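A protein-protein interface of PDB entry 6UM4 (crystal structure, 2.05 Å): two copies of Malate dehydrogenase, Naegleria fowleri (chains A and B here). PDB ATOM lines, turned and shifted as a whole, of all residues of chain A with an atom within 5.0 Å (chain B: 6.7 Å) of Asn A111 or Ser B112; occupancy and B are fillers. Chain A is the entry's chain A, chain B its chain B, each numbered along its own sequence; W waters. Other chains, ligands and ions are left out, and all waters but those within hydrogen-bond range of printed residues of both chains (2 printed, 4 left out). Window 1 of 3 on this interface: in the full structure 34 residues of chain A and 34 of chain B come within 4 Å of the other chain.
Of the 10 printed residues of chain A, 4 touch a printed residue of chain B. Hydrophobic or aromatic side chains of chain A within 4 Å of the printed part of chain B: Phe A115. Hydrophobic or aromatic side chains of chain B that line the printed part of chain A: Ala B333. Among the printed residues, 10 pairs touch across the chains.
Printed residues of chain B within 4 Å of Asn A111: Ser B112, Arg B327 and Ala B333. Printed residues of chain B within 4 Å of Glu A149: Arg B327, Ala B332, Ala B333 and Ser B334. Printed residues of chain A within 4 Å of Asn B111: Ser A112 (3.9 Å). Of the printed residues of chain A, Ser B112 touches Asn A111. Of the printed residues of chain A, Ala B332 touches Glu A149. Of the printed residues of chain A, Ala B333 touches Asn A111, Phe A115 and Glu A149. Of the printed residues of chain A, Ser B334 touches Glu A149 (2.8 Å). The nearest printed residue of chain B that does not touch Asn A111 is Asn B111 (4.8 Å). The nearest residue of chain A that does not touch Ser B112 is Ser A112 (4.6 Å).
The side-chain carboxylate (OE1) of Glu A149 is in salt-bridge range of the guanidinium group (NH2) of Arg B327 (2.5 Å). The side-chain hydroxyl (OG) of Ser B334 sits at hydrogen-bond distance from the side-chain carboxylate (OE2) of Glu A149 (2.8 Å).
Water W2 lies within hydrogen-bond range of OG of Ser B112 (3.1 Å) and O of Asn A111 (3.1 Å). Water W1 lies within hydrogen-bond range of the guanidinium group of Arg B327, the backbone NH of Asn A111 and the backbone carbonyl oxygen of Gly A107.
The side-chain carboxylate (OD1) of Asp B337 is in salt-bridge range of the guanidinium group (NH2) of Arg B116 (2.8 Å).
Asn A111 touches Ser B112, and with the chains exchanged Ser A112 touches Asn B111. Positions printed for both chains: 107, 108, 109, 110, 111, 112, 113, 114 and 115. Of the 10 pairs that touch across the chains among the printed residues, 2 have their exchanged pair printed and touching as well.
Among the printed residues, merely in contact across the chains: Phe A115 with Ala B333, Asn A111 with Ala B333, Glu A149 with Ala B333, Glu A149 with Ala B332, Asn A111 with Arg B327, Ser A112 with Asn B111, Asn A111 with Ser B112 and Phe A115 with Arg B116.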
ATOM      1  N   GLY A 107     -25.486 -34.812 -13.843  1.00  0.00           N
ATOM      2  CA  GLY A 107     -25.634 -34.459 -12.446  1.00  0.00           C
ATOM      3  C   GLY A 107     -25.686 -32.963 -12.175  1.00  0.00           C
ATOM      4  O   GLY A 107     -25.542 -32.112 -13.058  1.00  0.00           O
ATOM      5  N   GLN A 108     -25.885 -32.645 -10.888  1.00  0.00           N
ATOM      6  CA  GLN A 108     -26.070 -31.253 -10.484  1.00  0.00           C
ATOM      7  C   GLN A 108     -24.777 -30.457 -10.625  1.00  0.00           C
ATOM      8  O   GLN A 108     -24.795 -29.310 -11.096  1.00  0.00           O
ATOM      9  CB  GLN A 108     -26.606 -31.194  -9.056  1.00  0.00           C
ATOM     10  CG  GLN A 108     -28.067 -31.610  -8.948  1.00  0.00           C
ATOM     11  CD  GLN A 108     -28.971 -30.822  -9.883  1.00  0.00           C
ATOM     12  OE1 GLN A 108     -28.901 -29.590  -9.957  1.00  0.00           O
ATOM     13  NE2 GLN A 108     -29.814 -31.539 -10.624  1.00  0.00           N
ATOM     14  N   ILE A 109     -23.640 -31.069 -10.279  1.00  0.00           N
ATOM     15  CA  ILE A 109     -22.356 -30.404 -10.477  1.00  0.00           C
ATOM     16  C   ILE A 109     -22.135 -30.109 -11.960  1.00  0.00           C
ATOM     17  O   ILE A 109     -21.735 -28.998 -12.338  1.00  0.00           O
ATOM     18  CB  ILE A 109     -21.214 -31.257  -9.896  1.00  0.00           C
ATOM     19  CG1 ILE A 109     -21.217 -31.215  -8.354  1.00  0.00           C
ATOM     20  CG2 ILE A 109     -19.899 -30.805 -10.471  1.00  0.00           C
ATOM     21  CD1 ILE A 109     -20.204 -32.198  -7.733  1.00  0.00           C
ATOM     22  N   ALA A 110     -22.390 -31.098 -12.823  1.00  0.00           N
ATOM     23  CA  ALA A 110     -22.228 -30.876 -14.263  1.00  0.00           C
ATOM     24  C   ALA A 110     -23.108 -29.733 -14.764  1.00  0.00           C
ATOM     25  O   ALA A 110     -22.676 -28.931 -15.603  1.00  0.00           O
ATOM     26  CB  ALA A 110     -22.547 -32.154 -15.040  1.00  0.00           C
ATOM     27  N   ASN A 111     -24.339 -29.643 -14.259  1.00  0.00           N
ATOM     28  CA  ASN A 111     -25.260 -28.592 -14.714  1.00  0.00           C
ATOM     29  C   ASN A 111     -24.654 -27.196 -14.563  1.00  0.00           C
ATOM     30  O   ASN A 111     -24.889 -26.324 -15.411  1.00  0.00           O
ATOM     31  CB  ASN A 111     -26.588 -28.704 -13.957  1.00  0.00           C
ATOM     32  CG  ASN A 111     -27.574 -27.577 -14.300  1.00  0.00           C
ATOM     33  OD1 ASN A 111     -27.745 -26.626 -13.521  1.00  0.00           O
ATOM     34  ND2 ASN A 111     -28.255 -27.701 -15.433  1.00  0.00           N
ATOM     35  N   SER A 112     -23.841 -26.972 -13.524  1.00  0.00           N
ATOM     36  CA  SER A 112     -23.138 -25.703 -13.388  1.00  0.00           C
ATOM     37  C   SER A 112     -21.798 -25.699 -14.109  1.00  0.00           C
ATOM     38  O   SER A 112     -21.400 -24.663 -14.658  1.00  0.00           O
ATOM     39  CB  SER A 112     -22.943 -25.347 -11.907  1.00  0.00           C
ATOM     40  OG  SER A 112     -24.184 -25.019 -11.302  1.00  0.00           O
ATOM     41  N   LEU A 113     -21.104 -26.836 -14.143  1.00  0.00           N
ATOM     42  CA  LEU A 113     -19.760 -26.884 -14.717  1.00  0.00           C
ATOM     43  C   LEU A 113     -19.751 -26.622 -16.224  1.00  0.00           C
ATOM     44  O   LEU A 113     -18.903 -25.878 -16.739  1.00  0.00           O
ATOM     45  CB  LEU A 113     -19.139 -28.245 -14.432  1.00  0.00           C
ATOM     46  CG  LEU A 113     -17.739 -28.390 -14.989  1.00  0.00           C
ATOM     47  CD1 LEU A 113     -16.764 -27.804 -13.981  1.00  0.00           C
ATOM     48  CD2 LEU A 113     -17.431 -29.849 -15.244  1.00  0.00           C
ATOM     49  N   LEU A 114     -20.625 -27.293 -16.965  1.00  0.00           N
ATOM     50  CA  LEU A 114     -20.423 -27.340 -18.408  1.00  0.00           C
ATOM     51  C   LEU A 114     -20.581 -25.951 -19.029  1.00  0.00           C
ATOM     52  O   LEU A 114     -19.837 -25.594 -19.954  1.00  0.00           O
ATOM     53  CB  LEU A 114     -21.383 -28.353 -19.027  1.00  0.00           C
ATOM     54  CG  LEU A 114     -21.156 -29.798 -18.553  1.00  0.00           C
ATOM     55  CD1 LEU A 114     -22.246 -30.703 -19.129  1.00  0.00           C
ATOM     56  CD2 LEU A 114     -19.759 -30.336 -18.885  1.00  0.00           C
ATOM     57  N   PHE A 115     -21.529 -25.138 -18.518  1.00  0.00           N
ATOM     58  CA  PHE A 115     -21.717 -23.798 -19.066  1.00  0.00           C
ATOM     59  C   PHE A 115     -20.513 -22.901 -18.788  1.00  0.00           C
ATOM     60  O   PHE A 115     -20.198 -22.026 -19.603  1.00  0.00           O
ATOM     61  CB  PHE A 115     -23.008 -23.141 -18.521  1.00  0.00           C
ATOM     62  CG  PHE A 115     -24.285 -23.647 -19.158  1.00  0.00           C
ATOM     63  CD1 PHE A 115     -24.915 -22.921 -20.149  1.00  0.00           C
ATOM     64  CD2 PHE A 115     -24.836 -24.865 -18.773  1.00  0.00           C
ATOM     65  CE1 PHE A 115     -26.076 -23.391 -20.751  1.00  0.00           C
ATOM     66  CE2 PHE A 115     -25.975 -25.347 -19.361  1.00  0.00           C
ATOM     67  CZ  PHE A 115     -26.605 -24.609 -20.361  1.00  0.00           C
ATOM     68  N   GLU A 149     -29.632 -27.910 -23.822  1.00  0.00           N
ATOM     69  CA  GLU A 149     -29.463 -26.677 -23.056  1.00  0.00           C
ATOM     70  C   GLU A 149     -28.156 -25.995 -23.410  1.00  0.00           C
ATOM     71  O   GLU A 149     -28.107 -24.770 -23.546  1.00  0.00           O
ATOM     72  CB  GLU A 149     -29.531 -26.964 -21.559  1.00  0.00           C
ATOM     73  CG  GLU A 149     -30.924 -27.295 -21.048  1.00  0.00           C
ATOM     74  CD  GLU A 149     -31.172 -26.775 -19.620  1.00  0.00           C
ATOM     75  OE1 GLU A 149     -31.108 -27.606 -18.682  1.00  0.00           O
ATOM     76  OE2 GLU A 149     -31.391 -25.542 -19.434  1.00  0.00           O
ATOM     77  N   GLY B 107     -34.038 -19.946  -6.400  1.00  0.00           N
ATOM     78  CA  GLY B 107     -34.466 -20.856  -7.442  1.00  0.00           C
ATOM     79  C   GLY B 107     -33.325 -21.436  -8.264  1.00  0.00           C
ATOM     80  O   GLY B 107     -32.143 -21.141  -8.074  1.00  0.00           O
ATOM     81  N   GLN B 108     -33.709 -22.307  -9.199  1.00  0.00           N
ATOM     82  CA  GLN B 108     -32.731 -22.981 -10.050  1.00  0.00           C
ATOM     83  C   GLN B 108     -32.058 -22.012 -11.014  1.00  0.00           C
ATOM     84  O   GLN B 108     -30.871 -22.168 -11.323  1.00  0.00           O
ATOM     85  CB  GLN B 108     -33.403 -24.140 -10.789  1.00  0.00           C
ATOM     86  CG  GLN B 108     -33.558 -25.386  -9.936  1.00  0.00           C
ATOM     87  CD  GLN B 108     -32.203 -25.895  -9.441  1.00  0.00           C
ATOM     88  OE1 GLN B 108     -31.256 -26.026 -10.227  1.00  0.00           O
ATOM     89  NE2 GLN B 108     -32.094 -26.154  -8.136  1.00  0.00           N
ATOM     90  N   ILE B 109     -32.796 -21.028 -11.535  1.00  0.00           N
ATOM     91  CA  ILE B 109     -32.165 -20.046 -12.415  1.00  0.00           C
ATOM     92  C   ILE B 109     -31.144 -19.232 -11.646  1.00  0.00           C
ATOM     93  O   ILE B 109     -30.019 -19.023 -12.110  1.00  0.00           O
ATOM     94  CB  ILE B 109     -33.205 -19.142 -13.094  1.00  0.00           C
ATOM     95  CG1 ILE B 109     -34.006 -19.950 -14.114  1.00  0.00           C
ATOM     96  CG2 ILE B 109     -32.492 -18.030 -13.816  1.00  0.00           C
ATOM     97  CD1 ILE B 109     -35.142 -19.176 -14.734  1.00  0.00           C
ATOM     98  N   ALA B 110     -31.520 -18.756 -10.455  1.00  0.00           N
ATOM     99  CA  ALA B 110     -30.559 -18.037  -9.620  1.00  0.00           C
ATOM    100  C   ALA B 110     -29.337 -18.906  -9.325  1.00  0.00           C
ATOM    101  O   ALA B 110     -28.202 -18.412  -9.321  1.00  0.00           O
ATOM    102  CB  ALA B 110     -31.231 -17.580  -8.326  1.00  0.00           C
ATOM    103  N   ASN B 111     -29.548 -20.210  -9.095  1.00  0.00           N
ATOM    104  CA  ASN B 111     -28.438 -21.116  -8.789  1.00  0.00           C
ATOM    105  C   ASN B 111     -27.357 -21.083  -9.872  1.00  0.00           C
ATOM    106  O   ASN B 111     -26.161 -21.190  -9.568  1.00  0.00           O
ATOM    107  CB  ASN B 111     -28.962 -22.545  -8.606  1.00  0.00           C
ATOM    108  CG  ASN B 111     -27.843 -23.564  -8.373  1.00  0.00           C
ATOM    109  OD1 ASN B 111     -27.470 -24.313  -9.284  1.00  0.00           O
ATOM    110  ND2 ASN B 111     -27.326 -23.617  -7.152  1.00  0.00           N
ATOM    111  N   SER B 112     -27.753 -20.929 -11.140  1.00  0.00           N
ATOM    112  CA  SER B 112     -26.776 -20.773 -12.212  1.00  0.00           C
ATOM    113  C   SER B 112     -26.376 -19.319 -12.415  1.00  0.00           C
ATOM    114  O   SER B 112     -25.189 -19.041 -12.624  1.00  0.00           O
ATOM    115  CB  SER B 112     -27.336 -21.312 -13.530  1.00  0.00           C
ATOM    116  OG  SER B 112     -27.506 -22.706 -13.490  1.00  0.00           O
ATOM    117  N   LEU B 113     -27.342 -18.390 -12.281  1.00  0.00           N
ATOM    118  CA  LEU B 113     -27.102 -16.975 -12.581  1.00  0.00           C
ATOM    119  C   LEU B 113     -26.056 -16.358 -11.665  1.00  0.00           C
ATOM    120  O   LEU B 113     -25.145 -15.664 -12.133  1.00  0.00           O
ATOM    121  CB  LEU B 113     -28.395 -16.183 -12.440  1.00  0.00           C
ATOM    122  CG  LEU B 113     -28.333 -14.688 -12.745  1.00  0.00           C
ATOM    123  CD1 LEU B 113     -28.469 -14.465 -14.237  1.00  0.00           C
ATOM    124  CD2 LEU B 113     -29.448 -13.945 -12.041  1.00  0.00           C
ATOM    125  N   LEU B 114     -26.198 -16.567 -10.347  1.00  0.00           N
ATOM    126  CA  LEU B 114     -25.463 -15.764  -9.367  1.00  0.00           C
ATOM    127  C   LEU B 114     -23.956 -15.990  -9.461  1.00  0.00           C
ATOM    128  O   LEU B 114     -23.169 -15.042  -9.337  1.00  0.00           O
ATOM    129  CB  LEU B 114     -25.975 -16.078  -7.963  1.00  0.00           C
ATOM    130  CG  LEU B 114     -27.430 -15.679  -7.685  1.00  0.00           C
ATOM    131  CD1 LEU B 114     -27.890 -16.132  -6.319  1.00  0.00           C
ATOM    132  CD2 LEU B 114     -27.642 -14.181  -7.891  1.00  0.00           C
ATOM    133  N   PHE B 115     -23.535 -17.226  -9.708  1.00  0.00           N
ATOM    134  CA  PHE B 115     -22.106 -17.508  -9.822  1.00  0.00           C
ATOM    135  C   PHE B 115     -21.498 -16.835 -11.040  1.00  0.00           C
ATOM    136  O   PHE B 115     -20.319 -16.471 -11.016  1.00  0.00           O
ATOM    137  CB  PHE B 115     -21.892 -19.014  -9.870  1.00  0.00           C
ATOM    138  CG  PHE B 115     -22.000 -19.652  -8.534  1.00  0.00           C
ATOM    139  CD1 PHE B 115     -20.874 -20.044  -7.854  1.00  0.00           C
ATOM    140  CD2 PHE B 115     -23.234 -19.825  -7.939  1.00  0.00           C
ATOM    141  CE1 PHE B 115     -20.976 -20.594  -6.595  1.00  0.00           C
ATOM    142  CE2 PHE B 115     -23.333 -20.381  -6.687  1.00  0.00           C
ATOM    143  CZ  PHE B 115     -22.195 -20.772  -6.015  1.00  0.00           C
ATOM    144  N   ARG B 116     -22.288 -16.633 -12.091  1.00  0.00           N
ATOM    145  CA  ARG B 116     -21.822 -15.985 -13.308  1.00  0.00           C
ATOM    146  C   ARG B 116     -21.994 -14.469 -13.271  1.00  0.00           C
ATOM    147  O   ARG B 116     -21.583 -13.778 -14.211  1.00  0.00           O
ATOM    148  CB  ARG B 116     -22.539 -16.609 -14.509  1.00  0.00           C
ATOM    149  CG  ARG B 116     -22.177 -18.092 -14.674  1.00  0.00           C
ATOM    150  CD  ARG B 116     -22.958 -18.721 -15.825  1.00  0.00           C
ATOM    151  NE  ARG B 116     -22.526 -18.195 -17.104  1.00  0.00           N
ATOM    152  CZ  ARG B 116     -23.119 -18.501 -18.260  1.00  0.00           C
ATOM    153  NH1 ARG B 116     -24.166 -19.324 -18.286  1.00  0.00           N
ATOM    154  NH2 ARG B 116     -22.667 -17.986 -19.385  1.00  0.00           N
ATOM    155  N   ILE B 117     -22.576 -13.937 -12.203  1.00  0.00           N
ATOM    156  CA  ILE B 117     -22.373 -12.540 -11.843  1.00  0.00           C
ATOM    157  C   ILE B 117     -21.137 -12.385 -10.968  1.00  0.00           C
ATOM    158  O   ILE B 117     -20.274 -11.541 -11.217  1.00  0.00           O
ATOM    159  CB  ILE B 117     -23.625 -11.975 -11.133  1.00  0.00           C
ATOM    160  CG1 ILE B 117     -24.818 -11.906 -12.088  1.00  0.00           C
ATOM    161  CG2 ILE B 117     -23.320 -10.611 -10.582  1.00  0.00           C
ATOM    162  CD1 ILE B 117     -26.108 -11.649 -11.367  1.00  0.00           C
ATOM    163  N   ARG B 327     -35.303 -33.872 -19.941  1.00  0.00           N
ATOM    164  CA  ARG B 327     -34.688 -33.822 -18.619  1.00  0.00           C
ATOM    165  C   ARG B 327     -35.674 -34.014 -17.477  1.00  0.00           C
ATOM    166  O   ARG B 327     -35.259 -34.440 -16.395  1.00  0.00           O
ATOM    167  CB  ARG B 327     -33.959 -32.489 -18.417  1.00  0.00           C
ATOM    168  CG  ARG B 327     -32.873 -32.229 -19.440  1.00  0.00           C
ATOM    169  CD  ARG B 327     -31.966 -31.086 -19.023  1.00  0.00           C
ATOM    170  NE  ARG B 327     -31.047 -31.456 -17.953  1.00  0.00           N
ATOM    171  CZ  ARG B 327     -29.952 -30.757 -17.652  1.00  0.00           C
ATOM    172  NH1 ARG B 327     -29.160 -31.153 -16.664  1.00  0.00           N
ATOM    173  NH2 ARG B 327     -29.649 -29.657 -18.342  1.00  0.00           N
ATOM    174  N   ALA B 332     -33.380 -24.369 -16.532  1.00  0.00           N
ATOM    175  CA  ALA B 332     -32.859 -23.340 -15.636  1.00  0.00           C
ATOM    176  C   ALA B 332     -31.491 -22.821 -16.083  1.00  0.00           C
ATOM    177  O   ALA B 332     -31.240 -21.609 -16.063  1.00  0.00           O
ATOM    178  CB  ALA B 332     -32.789 -23.882 -14.215  1.00  0.00           C
ATOM    179  N   ALA B 333     -30.580 -23.716 -16.476  1.00  0.00           N
ATOM    180  CA  ALA B 333     -29.230 -23.267 -16.792  1.00  0.00           C
ATOM    181  C   ALA B 333     -29.214 -22.400 -18.048  1.00  0.00           C
ATOM    182  O   ALA B 333     -28.527 -21.370 -18.093  1.00  0.00           O
ATOM    183  CB  ALA B 333     -28.277 -24.467 -16.918  1.00  0.00           C
ATOM    184  N   SER B 334     -29.943 -22.787 -19.093  1.00  0.00           N
ATOM    185  CA  SER B 334     -29.905 -21.925 -20.262  1.00  0.00           C
ATOM    186  C   SER B 334     -30.679 -20.626 -20.019  1.00  0.00           C
ATOM    187  O   SER B 334     -30.288 -19.574 -20.533  1.00  0.00           O
ATOM    188  CB  SER B 334     -30.393 -22.680 -21.510  1.00  0.00           C
ATOM    189  OG  SER B 334     -31.562 -23.437 -21.272  1.00  0.00           O
ATOM    190  N   ALA B 336     -30.679 -18.946 -17.132  1.00  0.00           N
ATOM    191  CA  ALA B 336     -29.691 -18.090 -16.476  1.00  0.00           C
ATOM    192  C   ALA B 336     -28.668 -17.590 -17.483  1.00  0.00           C
ATOM    193  O   ALA B 336     -28.289 -16.413 -17.469  1.00  0.00           O
ATOM    194  CB  ALA B 336     -29.000 -18.833 -15.313  1.00  0.00           C
ATOM    195  N   ASP B 337     -28.233 -18.464 -18.393  1.00  0.00           N
ATOM    196  CA  ASP B 337     -27.274 -18.054 -19.414  1.00  0.00           C
ATOM    197  C   ASP B 337     -27.825 -16.914 -20.270  1.00  0.00           C
ATOM    198  O   ASP B 337     -27.122 -15.940 -20.565  1.00  0.00           O
ATOM    199  CB  ASP B 337     -26.905 -19.238 -20.305  1.00  0.00           C
ATOM    200  CG  ASP B 337     -25.940 -18.841 -21.385  1.00  0.00           C
ATOM    201  OD1 ASP B 337     -24.717 -18.835 -21.107  1.00  0.00           O
ATOM    202  OD2 ASP B 337     -26.402 -18.465 -22.487  1.00  0.00           O
ATOM    203  N   ILE B 340     -27.680 -13.702 -18.303  1.00  0.00           N
ATOM    204  CA  ILE B 340     -26.334 -13.144 -18.272  1.00  0.00           C
ATOM    205  C   ILE B 340     -26.042 -12.385 -19.559  1.00  0.00           C
ATOM    206  O   ILE B 340     -25.582 -11.234 -19.536  1.00  0.00           O
ATOM    207  CB  ILE B 340     -25.302 -14.265 -18.014  1.00  0.00           C
ATOM    208  CG1 ILE B 340     -25.485 -14.831 -16.611  1.00  0.00           C
ATOM    209  CG2 ILE B 340     -23.890 -13.729 -18.120  1.00  0.00           C
ATOM    210  CD1 ILE B 340     -25.148 -13.832 -15.466  1.00  0.00           C
HETATM  211  O   HOH W   1     -25.942 -31.677 -16.327  1.00  0.00           O
HETATM  212  O   HOH W   2     -25.181 -23.228 -15.463  1.00  0.00           O
